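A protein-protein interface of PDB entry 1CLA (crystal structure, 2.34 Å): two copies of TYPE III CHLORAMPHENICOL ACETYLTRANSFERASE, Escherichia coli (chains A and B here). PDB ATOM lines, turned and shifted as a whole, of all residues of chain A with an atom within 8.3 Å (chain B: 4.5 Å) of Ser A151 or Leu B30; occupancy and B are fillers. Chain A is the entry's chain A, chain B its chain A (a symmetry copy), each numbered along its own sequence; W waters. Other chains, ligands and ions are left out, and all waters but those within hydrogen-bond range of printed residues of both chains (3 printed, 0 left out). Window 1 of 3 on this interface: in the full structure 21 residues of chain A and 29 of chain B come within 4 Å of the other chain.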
ATOM      1  N   SER A  29      14.805  16.639  -4.053  1.00  0.00           N
ATOM      2  CA  SER A  29      13.749  16.466  -3.060  1.00  0.00           C
ATOM      3  C   SER A  29      13.365  17.904  -2.702  1.00  0.00           C
ATOM      4  O   SER A  29      14.202  18.828  -2.839  1.00  0.00           O
ATOM      5  CB  SER A  29      14.122  15.675  -1.826  1.00  0.00           C
ATOM      6  OG  SER A  29      15.211  16.272  -1.109  1.00  0.00           O
ATOM      7  N   LEU A  30      12.141  18.014  -2.301  1.00  0.00           N
ATOM      8  CA  LEU A  30      11.520  19.231  -1.758  1.00  0.00           C
ATOM      9  C   LEU A  30      10.430  18.790  -0.813  1.00  0.00           C
ATOM     10  O   LEU A  30       9.789  17.767  -1.001  1.00  0.00           O
ATOM     11  CB  LEU A  30      11.143  20.221  -2.861  1.00  0.00           C
ATOM     12  CG  LEU A  30       9.874  20.185  -3.624  1.00  0.00           C
ATOM     13  CD1 LEU A  30       8.664  20.611  -2.787  1.00  0.00           C
ATOM     14  CD2 LEU A  30       9.861  21.220  -4.760  1.00  0.00           C
ATOM     15  N   THR A  31      10.331  19.477   0.329  1.00  0.00           N
ATOM     16  CA  THR A  31       9.293  19.164   1.307  1.00  0.00           C
ATOM     17  C   THR A  31       8.412  20.437   1.344  1.00  0.00           C
ATOM     18  O   THR A  31       9.027  21.518   1.455  1.00  0.00           O
ATOM     19  CB  THR A  31       9.735  19.037   2.801  1.00  0.00           C
ATOM     20  OG1 THR A  31      10.895  18.084   2.653  1.00  0.00           O
ATOM     21  CG2 THR A  31       8.783  18.546   3.818  1.00  0.00           C
ATOM     22  N   SER A  32       7.132  20.201   1.274  1.00  0.00           N
ATOM     23  CA  SER A  32       6.212  21.351   1.263  1.00  0.00           C
ATOM     24  C   SER A  32       5.161  21.059   2.315  1.00  0.00           C
ATOM     25  O   SER A  32       5.065  19.869   2.655  1.00  0.00           O
ATOM     26  CB  SER A  32       5.662  21.498  -0.151  1.00  0.00           C
ATOM     27  OG  SER A  32       4.660  22.482  -0.132  1.00  0.00           O
ATOM     28  N   LYS A  33       4.449  22.027   2.814  1.00  0.00           N
ATOM     29  CA  LYS A  33       3.364  21.755   3.739  1.00  0.00           C
ATOM     30  C   LYS A  33       2.035  21.820   2.974  1.00  0.00           C
ATOM     31  O   LYS A  33       1.732  22.778   2.247  1.00  0.00           O
ATOM     32  CB  LYS A  33       3.441  22.548   4.982  1.00  0.00           C
ATOM     33  CG  LYS A  33       4.705  22.164   5.847  1.00  0.00           C
ATOM     34  CD  LYS A  33       4.593  23.069   7.095  1.00  0.00           C
ATOM     35  CE  LYS A  33       5.514  22.566   8.219  1.00  0.00           C
ATOM     36  NZ  LYS A  33       6.833  22.343   7.584  1.00  0.00           N
ATOM     37  N   LEU A 144       6.140   8.868   8.416  1.00  0.00           N
ATOM     38  CA  LEU A 144       6.789   9.069   9.693  1.00  0.00           C
ATOM     39  C   LEU A 144       5.754   9.766  10.590  1.00  0.00           C
ATOM     40  O   LEU A 144       5.863  10.962  10.826  1.00  0.00           O
ATOM     41  CB  LEU A 144       8.111   9.809   9.600  1.00  0.00           C
ATOM     42  CG  LEU A 144       9.356   9.075   9.173  1.00  0.00           C
ATOM     43  CD1 LEU A 144       9.322   8.860   7.663  1.00  0.00           C
ATOM     44  CD2 LEU A 144      10.623   9.878   9.482  1.00  0.00           C
ATOM     45  N   TRP A 146       5.285   9.675  13.910  1.00  0.00           N
ATOM     46  CA  TRP A 146       5.727   9.995  15.248  1.00  0.00           C
ATOM     47  C   TRP A 146       6.414  11.331  15.390  1.00  0.00           C
ATOM     48  O   TRP A 146       6.786  11.644  16.548  1.00  0.00           O
ATOM     49  CB  TRP A 146       6.576   8.846  15.812  1.00  0.00           C
ATOM     50  CG  TRP A 146       6.273   7.487  15.321  1.00  0.00           C
ATOM     51  CD1 TRP A 146       5.388   6.627  15.899  1.00  0.00           C
ATOM     52  CD2 TRP A 146       6.750   6.843  14.147  1.00  0.00           C
ATOM     53  NE1 TRP A 146       5.251   5.466  15.107  1.00  0.00           N
ATOM     54  CE2 TRP A 146       6.074   5.564  14.066  1.00  0.00           C
ATOM     55  CE3 TRP A 146       7.616   7.187  13.119  1.00  0.00           C
ATOM     56  CZ2 TRP A 146       6.320   4.648  13.044  1.00  0.00           C
ATOM     57  CZ3 TRP A 146       7.874   6.270  12.120  1.00  0.00           C
ATOM     58  CH2 TRP A 146       7.270   4.998  12.097  1.00  0.00           C
ATOM     59  N   VAL A 147       6.727  12.110  14.425  1.00  0.00           N
ATOM     60  CA  VAL A 147       7.486  13.341  14.537  1.00  0.00           C
ATOM     61  C   VAL A 147       7.178  14.123  13.258  1.00  0.00           C
ATOM     62  O   VAL A 147       6.959  13.540  12.190  1.00  0.00           O
ATOM     63  CB  VAL A 147       9.012  13.053  14.665  1.00  0.00           C
ATOM     64  CG1 VAL A 147       9.604  12.531  13.348  1.00  0.00           C
ATOM     65  CG2 VAL A 147       9.795  14.267  15.111  1.00  0.00           C
ATOM     66  N   ASN A 148       7.202  15.391  13.413  1.00  0.00           N
ATOM     67  CA  ASN A 148       6.948  16.424  12.422  1.00  0.00           C
ATOM     68  C   ASN A 148       8.351  16.792  11.952  1.00  0.00           C
ATOM     69  O   ASN A 148       9.273  16.731  12.793  1.00  0.00           O
ATOM     70  CB  ASN A 148       6.266  17.631  13.091  1.00  0.00           C
ATOM     71  CG  ASN A 148       5.966  18.761  12.108  1.00  0.00           C
ATOM     72  OD1 ASN A 148       6.814  19.668  12.076  1.00  0.00           O
ATOM     73  ND2 ASN A 148       4.838  18.719  11.409  1.00  0.00           N
ATOM     74  N   PHE A 149       8.445  17.113  10.709  1.00  0.00           N
ATOM     75  CA  PHE A 149       9.767  17.424  10.151  1.00  0.00           C
ATOM     76  C   PHE A 149       9.418  18.553   9.136  1.00  0.00           C
ATOM     77  O   PHE A 149       8.288  18.563   8.646  1.00  0.00           O
ATOM     78  CB  PHE A 149      10.508  16.236   9.562  1.00  0.00           C
ATOM     79  CG  PHE A 149       9.926  15.486   8.379  1.00  0.00           C
ATOM     80  CD1 PHE A 149       9.506  16.077   7.201  1.00  0.00           C
ATOM     81  CD2 PHE A 149       9.873  14.070   8.430  1.00  0.00           C
ATOM     82  CE1 PHE A 149       8.912  15.434   6.142  1.00  0.00           C
ATOM     83  CE2 PHE A 149       9.256  13.383   7.364  1.00  0.00           C
ATOM     84  CZ  PHE A 149       8.750  14.038   6.217  1.00  0.00           C
ATOM     85  N   ASP A 150      10.431  19.387   8.874  1.00  0.00           N
ATOM     86  CA  ASP A 150      10.333  20.451   7.916  1.00  0.00           C
ATOM     87  C   ASP A 150      11.036  19.961   6.640  1.00  0.00           C
ATOM     88  O   ASP A 150      10.792  20.626   5.635  1.00  0.00           O
ATOM     89  CB  ASP A 150      10.939  21.789   8.435  1.00  0.00           C
ATOM     90  CG  ASP A 150      10.141  22.189   9.684  1.00  0.00           C
ATOM     91  OD1 ASP A 150       9.039  22.602   9.402  1.00  0.00           O
ATOM     92  OD2 ASP A 150      10.557  22.062  10.874  1.00  0.00           O
ATOM     93  N   SER A 151      11.893  18.961   6.727  1.00  0.00           N
ATOM     94  CA  SER A 151      12.542  18.515   5.556  1.00  0.00           C
ATOM     95  C   SER A 151      12.882  17.028   5.726  1.00  0.00           C
ATOM     96  O   SER A 151      13.224  16.720   6.876  1.00  0.00           O
ATOM     97  CB  SER A 151      13.891  19.174   5.264  1.00  0.00           C
ATOM     98  OG  SER A 151      14.922  18.644   6.030  1.00  0.00           O
ATOM     99  N   PHE A 152      12.924  16.292   4.618  1.00  0.00           N
ATOM    100  CA  PHE A 152      13.339  14.879   4.613  1.00  0.00           C
ATOM    101  C   PHE A 152      14.117  14.665   3.327  1.00  0.00           C
ATOM    102  O   PHE A 152      13.609  15.173   2.312  1.00  0.00           O
ATOM    103  CB  PHE A 152      12.157  13.929   4.691  1.00  0.00           C
ATOM    104  CG  PHE A 152      12.483  12.473   4.698  1.00  0.00           C
ATOM    105  CD1 PHE A 152      12.667  11.830   5.930  1.00  0.00           C
ATOM    106  CD2 PHE A 152      12.592  11.779   3.492  1.00  0.00           C
ATOM    107  CE1 PHE A 152      12.910  10.453   6.002  1.00  0.00           C
ATOM    108  CE2 PHE A 152      12.824  10.372   3.530  1.00  0.00           C
ATOM    109  CZ  PHE A 152      13.002   9.731   4.783  1.00  0.00           C
ATOM    110  N   ASN A 153      15.221  13.974   3.287  1.00  0.00           N
ATOM    111  CA  ASN A 153      15.901  13.717   2.019  1.00  0.00           C
ATOM    112  C   ASN A 153      16.518  12.326   2.155  1.00  0.00           C
ATOM    113  O   ASN A 153      17.172  12.162   3.183  1.00  0.00           O
ATOM    114  CB  ASN A 153      16.872  14.844   1.689  1.00  0.00           C
ATOM    115  CG  ASN A 153      17.725  14.538   0.449  1.00  0.00           C
ATOM    116  OD1 ASN A 153      18.863  13.988   0.558  1.00  0.00           O
ATOM    117  ND2 ASN A 153      17.245  14.801  -0.773  1.00  0.00           N
ATOM    118  N   LEU A 154      16.379  11.463   1.194  1.00  0.00           N
ATOM    119  CA  LEU A 154      16.991  10.116   1.055  1.00  0.00           C
ATOM    120  C   LEU A 154      18.332  10.304   0.332  1.00  0.00           C
ATOM    121  O   LEU A 154      18.340  10.928  -0.742  1.00  0.00           O
ATOM    122  CB  LEU A 154      16.104   9.157   0.350  1.00  0.00           C
ATOM    123  CG  LEU A 154      15.024   8.556   1.279  1.00  0.00           C
ATOM    124  CD1 LEU A 154      13.974   7.956   0.350  1.00  0.00           C
ATOM    125  CD2 LEU A 154      15.733   7.477   2.083  1.00  0.00           C
ATOM    126  N   ASN A 155      19.434   9.908   0.915  1.00  0.00           N
ATOM    127  CA  ASN A 155      20.763  10.051   0.304  1.00  0.00           C
ATOM    128  C   ASN A 155      21.004   8.606  -0.192  1.00  0.00           C
ATOM    129  O   ASN A 155      21.114   7.698   0.704  1.00  0.00           O
ATOM    130  CB  ASN A 155      21.701  10.537   1.379  1.00  0.00           C
ATOM    131  CG  ASN A 155      21.404  11.963   1.859  1.00  0.00           C
ATOM    132  OD1 ASN A 155      21.100  12.237   3.041  1.00  0.00           O
ATOM    133  ND2 ASN A 155      21.541  12.907   0.955  1.00  0.00           N
ATOM    134  N   THR A 168       7.117  11.051   1.063  1.00  0.00           N
ATOM    135  CA  THR A 168       7.204  10.731   2.494  1.00  0.00           C
ATOM    136  C   THR A 168       6.385  11.794   3.266  1.00  0.00           C
ATOM    137  O   THR A 168       6.555  12.985   3.035  1.00  0.00           O
ATOM    138  CB  THR A 168       8.617  10.734   3.074  1.00  0.00           C
ATOM    139  OG1 THR A 168       9.525   9.821   2.309  1.00  0.00           O
ATOM    140  CG2 THR A 168       8.893  10.409   4.531  1.00  0.00           C
ATOM    141  N   ALA A 170       5.076  13.283   7.169  1.00  0.00           N
ATOM    142  CA  ALA A 170       5.464  13.353   8.619  1.00  0.00           C
ATOM    143  C   ALA A 170       4.156  13.566   9.408  1.00  0.00           C
ATOM    144  O   ALA A 170       3.066  13.663   8.826  1.00  0.00           O
ATOM    145  CB  ALA A 170       6.428  14.519   8.846  1.00  0.00           C
ATOM    146  N   PRO A 182       3.458  18.007   6.404  1.00  0.00           N
ATOM    147  CA  PRO A 182       4.749  18.006   5.728  1.00  0.00           C
ATOM    148  C   PRO A 182       4.802  16.833   4.730  1.00  0.00           C
ATOM    149  O   PRO A 182       4.544  15.679   5.123  1.00  0.00           O
ATOM    150  CB  PRO A 182       5.806  17.782   6.805  1.00  0.00           C
ATOM    151  CG  PRO A 182       5.136  18.035   8.129  1.00  0.00           C
ATOM    152  CD  PRO A 182       3.663  17.631   7.824  1.00  0.00           C
ATOM    153  N   LEU A 183       5.204  17.109   3.504  1.00  0.00           N
ATOM    154  CA  LEU A 183       5.233  16.114   2.436  1.00  0.00           C
ATOM    155  C   LEU A 183       6.511  16.353   1.602  1.00  0.00           C
ATOM    156  O   LEU A 183       6.650  17.436   1.002  1.00  0.00           O
ATOM    157  CB  LEU A 183       3.976  16.279   1.583  1.00  0.00           C
ATOM    158  CG  LEU A 183       3.632  15.207   0.560  1.00  0.00           C
ATOM    159  CD1 LEU A 183       2.467  14.383   1.109  1.00  0.00           C
ATOM    160  CD2 LEU A 183       3.168  15.906  -0.706  1.00  0.00           C
ATOM    161  N   SER A 184       7.359  15.349   1.698  1.00  0.00           N
ATOM    162  CA  SER A 184       8.629  15.337   0.977  1.00  0.00           C
ATOM    163  C   SER A 184       8.338  14.521  -0.309  1.00  0.00           C
ATOM    164  O   SER A 184       7.800  13.458  -0.253  1.00  0.00           O
ATOM    165  CB  SER A 184       9.775  14.750   1.766  1.00  0.00           C
ATOM    166  OG  SER A 184      10.973  14.986   1.025  1.00  0.00           O
ATOM    167  N   PHE B  28      19.285   8.840   5.258  1.00  0.00           N
ATOM    168  CA  PHE B  28      18.285   9.924   5.173  1.00  0.00           C
ATOM    169  C   PHE B  28      18.649  10.953   6.268  1.00  0.00           C
ATOM    170  O   PHE B  28      19.370  10.708   7.251  1.00  0.00           O
ATOM    171  CB  PHE B  28      16.893   9.304   5.293  1.00  0.00           C
ATOM    172  CG  PHE B  28      16.458   8.740   6.565  1.00  0.00           C
ATOM    173  CD1 PHE B  28      15.998   9.553   7.588  1.00  0.00           C
ATOM    174  CD2 PHE B  28      16.516   7.369   6.762  1.00  0.00           C
ATOM    175  CE1 PHE B  28      15.584   9.006   8.778  1.00  0.00           C
ATOM    176  CE2 PHE B  28      16.127   6.766   7.932  1.00  0.00           C
ATOM    177  CZ  PHE B  28      15.632   7.634   8.965  1.00  0.00           C
ATOM    178  N   SER B  29      18.152  12.138   6.051  1.00  0.00           N
ATOM    179  CA  SER B  29      18.256  13.282   6.953  1.00  0.00           C
ATOM    180  C   SER B  29      16.806  13.751   7.094  1.00  0.00           C
ATOM    181  O   SER B  29      15.980  13.517   6.178  1.00  0.00           O
ATOM    182  CB  SER B  29      19.154  14.408   6.493  1.00  0.00           C
ATOM    183  OG  SER B  29      18.732  14.963   5.241  1.00  0.00           O
ATOM    184  N   LEU B  30      16.577  14.348   8.217  1.00  0.00           N
ATOM    185  CA  LEU B  30      15.328  15.031   8.588  1.00  0.00           C
ATOM    186  C   LEU B  30      15.692  16.122   9.565  1.00  0.00           C
ATOM    187  O   LEU B  30      16.619  16.001  10.350  1.00  0.00           O
ATOM    188  CB  LEU B  30      14.239  14.041   9.005  1.00  0.00           C
ATOM    189  CG  LEU B  30      14.082  13.493  10.372  1.00  0.00           C
ATOM    190  CD1 LEU B  30      13.566  14.528  11.375  1.00  0.00           C
ATOM    191  CD2 LEU B  30      12.989  12.413  10.433  1.00  0.00           C
ATOM    192  N   THR B  31      15.065  17.289   9.398  1.00  0.00           N
ATOM    193  CA  THR B  31      15.309  18.411  10.303  1.00  0.00           C
ATOM    194  C   THR B  31      13.945  18.636  11.002  1.00  0.00           C
ATOM    195  O   THR B  31      12.952  18.687  10.246  1.00  0.00           O
ATOM    196  CB  THR B  31      15.572  19.807   9.653  1.00  0.00           C
ATOM    197  OG1 THR B  31      16.645  19.437   8.659  1.00  0.00           O
ATOM    198  CG2 THR B  31      16.007  20.945  10.490  1.00  0.00           C
ATOM    199  N   SER B  32      14.026  18.765  12.296  1.00  0.00           N
ATOM    200  CA  SER B  32      12.777  18.947  13.055  1.00  0.00           C
ATOM    201  C   SER B  32      13.003  20.143  13.958  1.00  0.00           C
ATOM    202  O   SER B  32      14.192  20.448  14.148  1.00  0.00           O
ATOM    203  CB  SER B  32      12.485  17.647  13.795  1.00  0.00           C
ATOM    204  OG  SER B  32      11.393  17.864  14.652  1.00  0.00           O
ATOM    205  N   ASP B 150      15.656  25.697   7.983  1.00  0.00           N
ATOM    206  CA  ASP B 150      14.535  24.809   8.096  1.00  0.00           C
ATOM    207  C   ASP B 150      15.029  23.418   7.666  1.00  0.00           C
ATOM    208  O   ASP B 150      14.285  22.492   7.978  1.00  0.00           O
ATOM    209  CB  ASP B 150      13.309  25.273   7.254  1.00  0.00           C
ATOM    210  CG  ASP B 150      12.891  26.650   7.791  1.00  0.00           C
ATOM    211  OD1 ASP B 150      12.336  26.564   8.864  1.00  0.00           O
ATOM    212  OD2 ASP B 150      13.133  27.751   7.215  1.00  0.00           O
ATOM    213  N   SER B 151      16.127  23.328   6.938  1.00  0.00           N
ATOM    214  CA  SER B 151      16.578  22.051   6.540  1.00  0.00           C
ATOM    215  C   SER B 151      18.102  22.107   6.366  1.00  0.00           C
ATOM    216  O   SER B 151      18.514  23.174   5.891  1.00  0.00           O
ATOM    217  CB  SER B 151      16.066  21.571   5.180  1.00  0.00           C
ATOM    218  OG  SER B 151      16.757  22.139   4.118  1.00  0.00           O
ATOM    219  N   LEU B 183      16.993  21.158  14.226  1.00  0.00           N
ATOM    220  CA  LEU B 183      17.921  20.062  14.487  1.00  0.00           C
ATOM    221  C   LEU B 183      17.786  19.042  13.335  1.00  0.00           C
ATOM    222  O   LEU B 183      16.695  18.470  13.155  1.00  0.00           O
ATOM    223  CB  LEU B 183      17.561  19.430  15.830  1.00  0.00           C
ATOM    224  CG  LEU B 183      18.525  18.435  16.461  1.00  0.00           C
ATOM    225  CD1 LEU B 183      19.236  19.133  17.620  1.00  0.00           C
ATOM    226  CD2 LEU B 183      17.704  17.288  17.025  1.00  0.00           C
ATOM    227  N   SER B 184      18.887  18.963  12.614  1.00  0.00           N
ATOM    228  CA  SER B 184      19.006  18.046  11.483  1.00  0.00           C
ATOM    229  C   SER B 184      19.708  16.794  12.070  1.00  0.00           C
ATOM    230  O   SER B 184      20.701  16.895  12.721  1.00  0.00           O
ATOM    231  CB  SER B 184      19.768  18.617  10.311  1.00  0.00           C
ATOM    232  OG  SER B 184      19.633  17.702   9.222  1.00  0.00           O
ATOM    233  N   VAL B 185      19.196  15.632  11.736  1.00  0.00           N
ATOM    234  CA  VAL B 185      19.652  14.267  12.103  1.00  0.00           C
ATOM    235  C   VAL B 185      19.898  13.538  10.781  1.00  0.00           C
ATOM    236  O   VAL B 185      18.931  13.493   9.996  1.00  0.00           O
ATOM    237  CB  VAL B 185      18.612  13.506  12.980  1.00  0.00           C
ATOM    238  CG1 VAL B 185      19.159  12.145  13.429  1.00  0.00           C
ATOM    239  CG2 VAL B 185      18.298  14.221  14.284  1.00  0.00           C
ATOM    240  N   VAL B 197      14.647   7.429  14.471  1.00  0.00           N
ATOM    241  CA  VAL B 197      14.944   8.849  14.396  1.00  0.00           C
ATOM    242  C   VAL B 197      13.885   9.645  15.164  1.00  0.00           C
ATOM    243  O   VAL B 197      14.255  10.520  15.960  1.00  0.00           O
ATOM    244  CB  VAL B 197      15.211   9.354  12.969  1.00  0.00           C
ATOM    245  CG1 VAL B 197      15.440  10.900  13.007  1.00  0.00           C
ATOM    246  CG2 VAL B 197      16.473   8.746  12.379  1.00  0.00           C
ATOM    247  N   ILE B 201      14.437  11.992  18.675  1.00  0.00           N
ATOM    248  CA  ILE B 201      13.989  13.392  18.701  1.00  0.00           C
ATOM    249  C   ILE B 201      13.004  13.597  19.852  1.00  0.00           C
ATOM    250  O   ILE B 201      13.114  14.522  20.709  1.00  0.00           O
ATOM    251  CB  ILE B 201      13.500  13.779  17.281  1.00  0.00           C
ATOM    252  CG1 ILE B 201      14.760  13.938  16.355  1.00  0.00           C
ATOM    253  CG2 ILE B 201      12.588  15.014  17.246  1.00  0.00           C
ATOM    254  CD1 ILE B 201      14.483  13.689  14.872  1.00  0.00           C
HETATM  255  O   HOH W   1      13.270  22.816  10.899  1.00  0.00           O
HETATM  256  O   HOH W   2      16.714  16.913   5.302  1.00  0.00           O
HETATM  257  O   HOH W   3      22.140  10.067   5.079  1.00  0.00           O
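The backbone carbonyl oxygen (O) of Phe A152 sits at hydrogen-bond distance from the side-chain hydroxyl (OG) of Ser A184 (2.9 Å).
The backbone carbonyl oxygen of Leu B30 sits at hydrogen-bond distance from the backbone NH of Val B185, 2.9 Å away.
OG1 of Thr A31 is in hydrogen-bond range of N of Phe A152 (3.3 Å).
NZ of Lys A33 lies within salt-bridge range of OD1 of Asp A150 (2.9 Å).
OD1 of Asn A153 sits at hydrogen-bond distance from ND2 of Asn A155.
The backbone NH (N) of Ser B32 lies within hydrogen-bond range of the backbone carbonyl oxygen (O) of Leu B183 (2.8 Å).
Water W2 lies within hydrogen-bond range of the side-chain hydroxyl (OG) of Ser A151 and the side-chain hydroxyl (OG) of Ser B29.
Water W1 bridges the side-chain carboxylate (OD2) of Asp A150 (2.8 Å) and the backbone carbonyl oxygen (O) of Asp B150 (3.1 Å).
Water W3 lies within hydrogen-bond range of N of Phe B28 (3.1 Å) and OD1 of Asn A155 (3.2 Å).
The backbone carbonyl oxygen of Ser B29 sits at hydrogen-bond distance from the backbone NH of Asn A153 (3.0 Å).
OG of Ser B32 lies within hydrogen-bond range of O of Asn A148, at 3.0 Å.
N of Asp A150 lies within hydrogen-bond range of O of Thr B31, at 3.0 Å.
N of Thr B31 is in hydrogen-bond range of O of Ser A151.
Among the printed residues, pairs that only touch across the chains: Leu A144 with Leu B30, Val A147 with Ser B32, Val A147 with Ile B201, Phe A149 with Leu B30, Phe A149 with Thr B31, Asp A150 with Asp B150, Ser A151 with Leu B30, Ser A151 with Ser B151, Phe A152 with Phe B28, Phe A152 with Ser B29, Asn A153 with Phe B28 and Leu A154 with Phe B28.
Printed residues of chain A that touch a printed residue of chain B: Leu A144, Val A147, Asn A148, Phe A149, Asp A150, Ser A151, Phe A152, Asn A153 and Leu A154.
Hydrophobic or aromatic side chains of chain A within 4 Å of the printed part of chain B: Leu A144, Val A147, Phe A149, Phe A152 and Leu A154.
Hydrophobic or aromatic side chains of chain B that line the printed part of chain A: Phe B28, Leu B30 and Ile B201.
Of the printed residues of chain B, Asp A150 touches Thr B31 and Asp B150.
Ser A151 touches three residues of chain B.
Of the printed residues of chain B, Phe A152 touches Phe B28 (3.6 Å) and Ser B29 (3.4 Å).
Printed residues of chain B within 4 Å of Asn A153: Phe B28 (3.2 Å) and Ser B29 (3.0 Å).
Asn A155 touches none of the printed residues of chain B.
Of the printed residues of chain A, Ser B151 touches Ser A151 (3.2 Å).
Val B197 touches none of the printed residues of chain A.
Of the printed residues of chain A, Ile B201 touches Val A147 (3.6 Å).
The nearest printed residue of chain B that does not touch Ser A151 is Ser B29 (4.3 Å).
The nearest residue of chain A that does not touch Leu B30 is Phe A152 (4.1 Å).
The nearest printed residue of chain B that does not touch Asp A150 is Ser B32 (4.4 Å).
Asp A150 touches Thr B31, but with the chains exchanged Thr A31 does not touch Asp B150 (7.7 Å).
Asp B150 touches its own counterpart, Asp A150.
Ser A151 touches Leu B30, but with the chains exchanged Leu A30 does not touch Ser B151 (8.4 Å).
Ser A151 touches Thr B31, but with the chains exchanged Thr A31 does not touch Ser B151 (6.7 Å).
8 positions are printed for both chains.
Of the 16 pairs that touch across the chains among the printed residues, 2 have their exchanged pair printed and touching as well.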
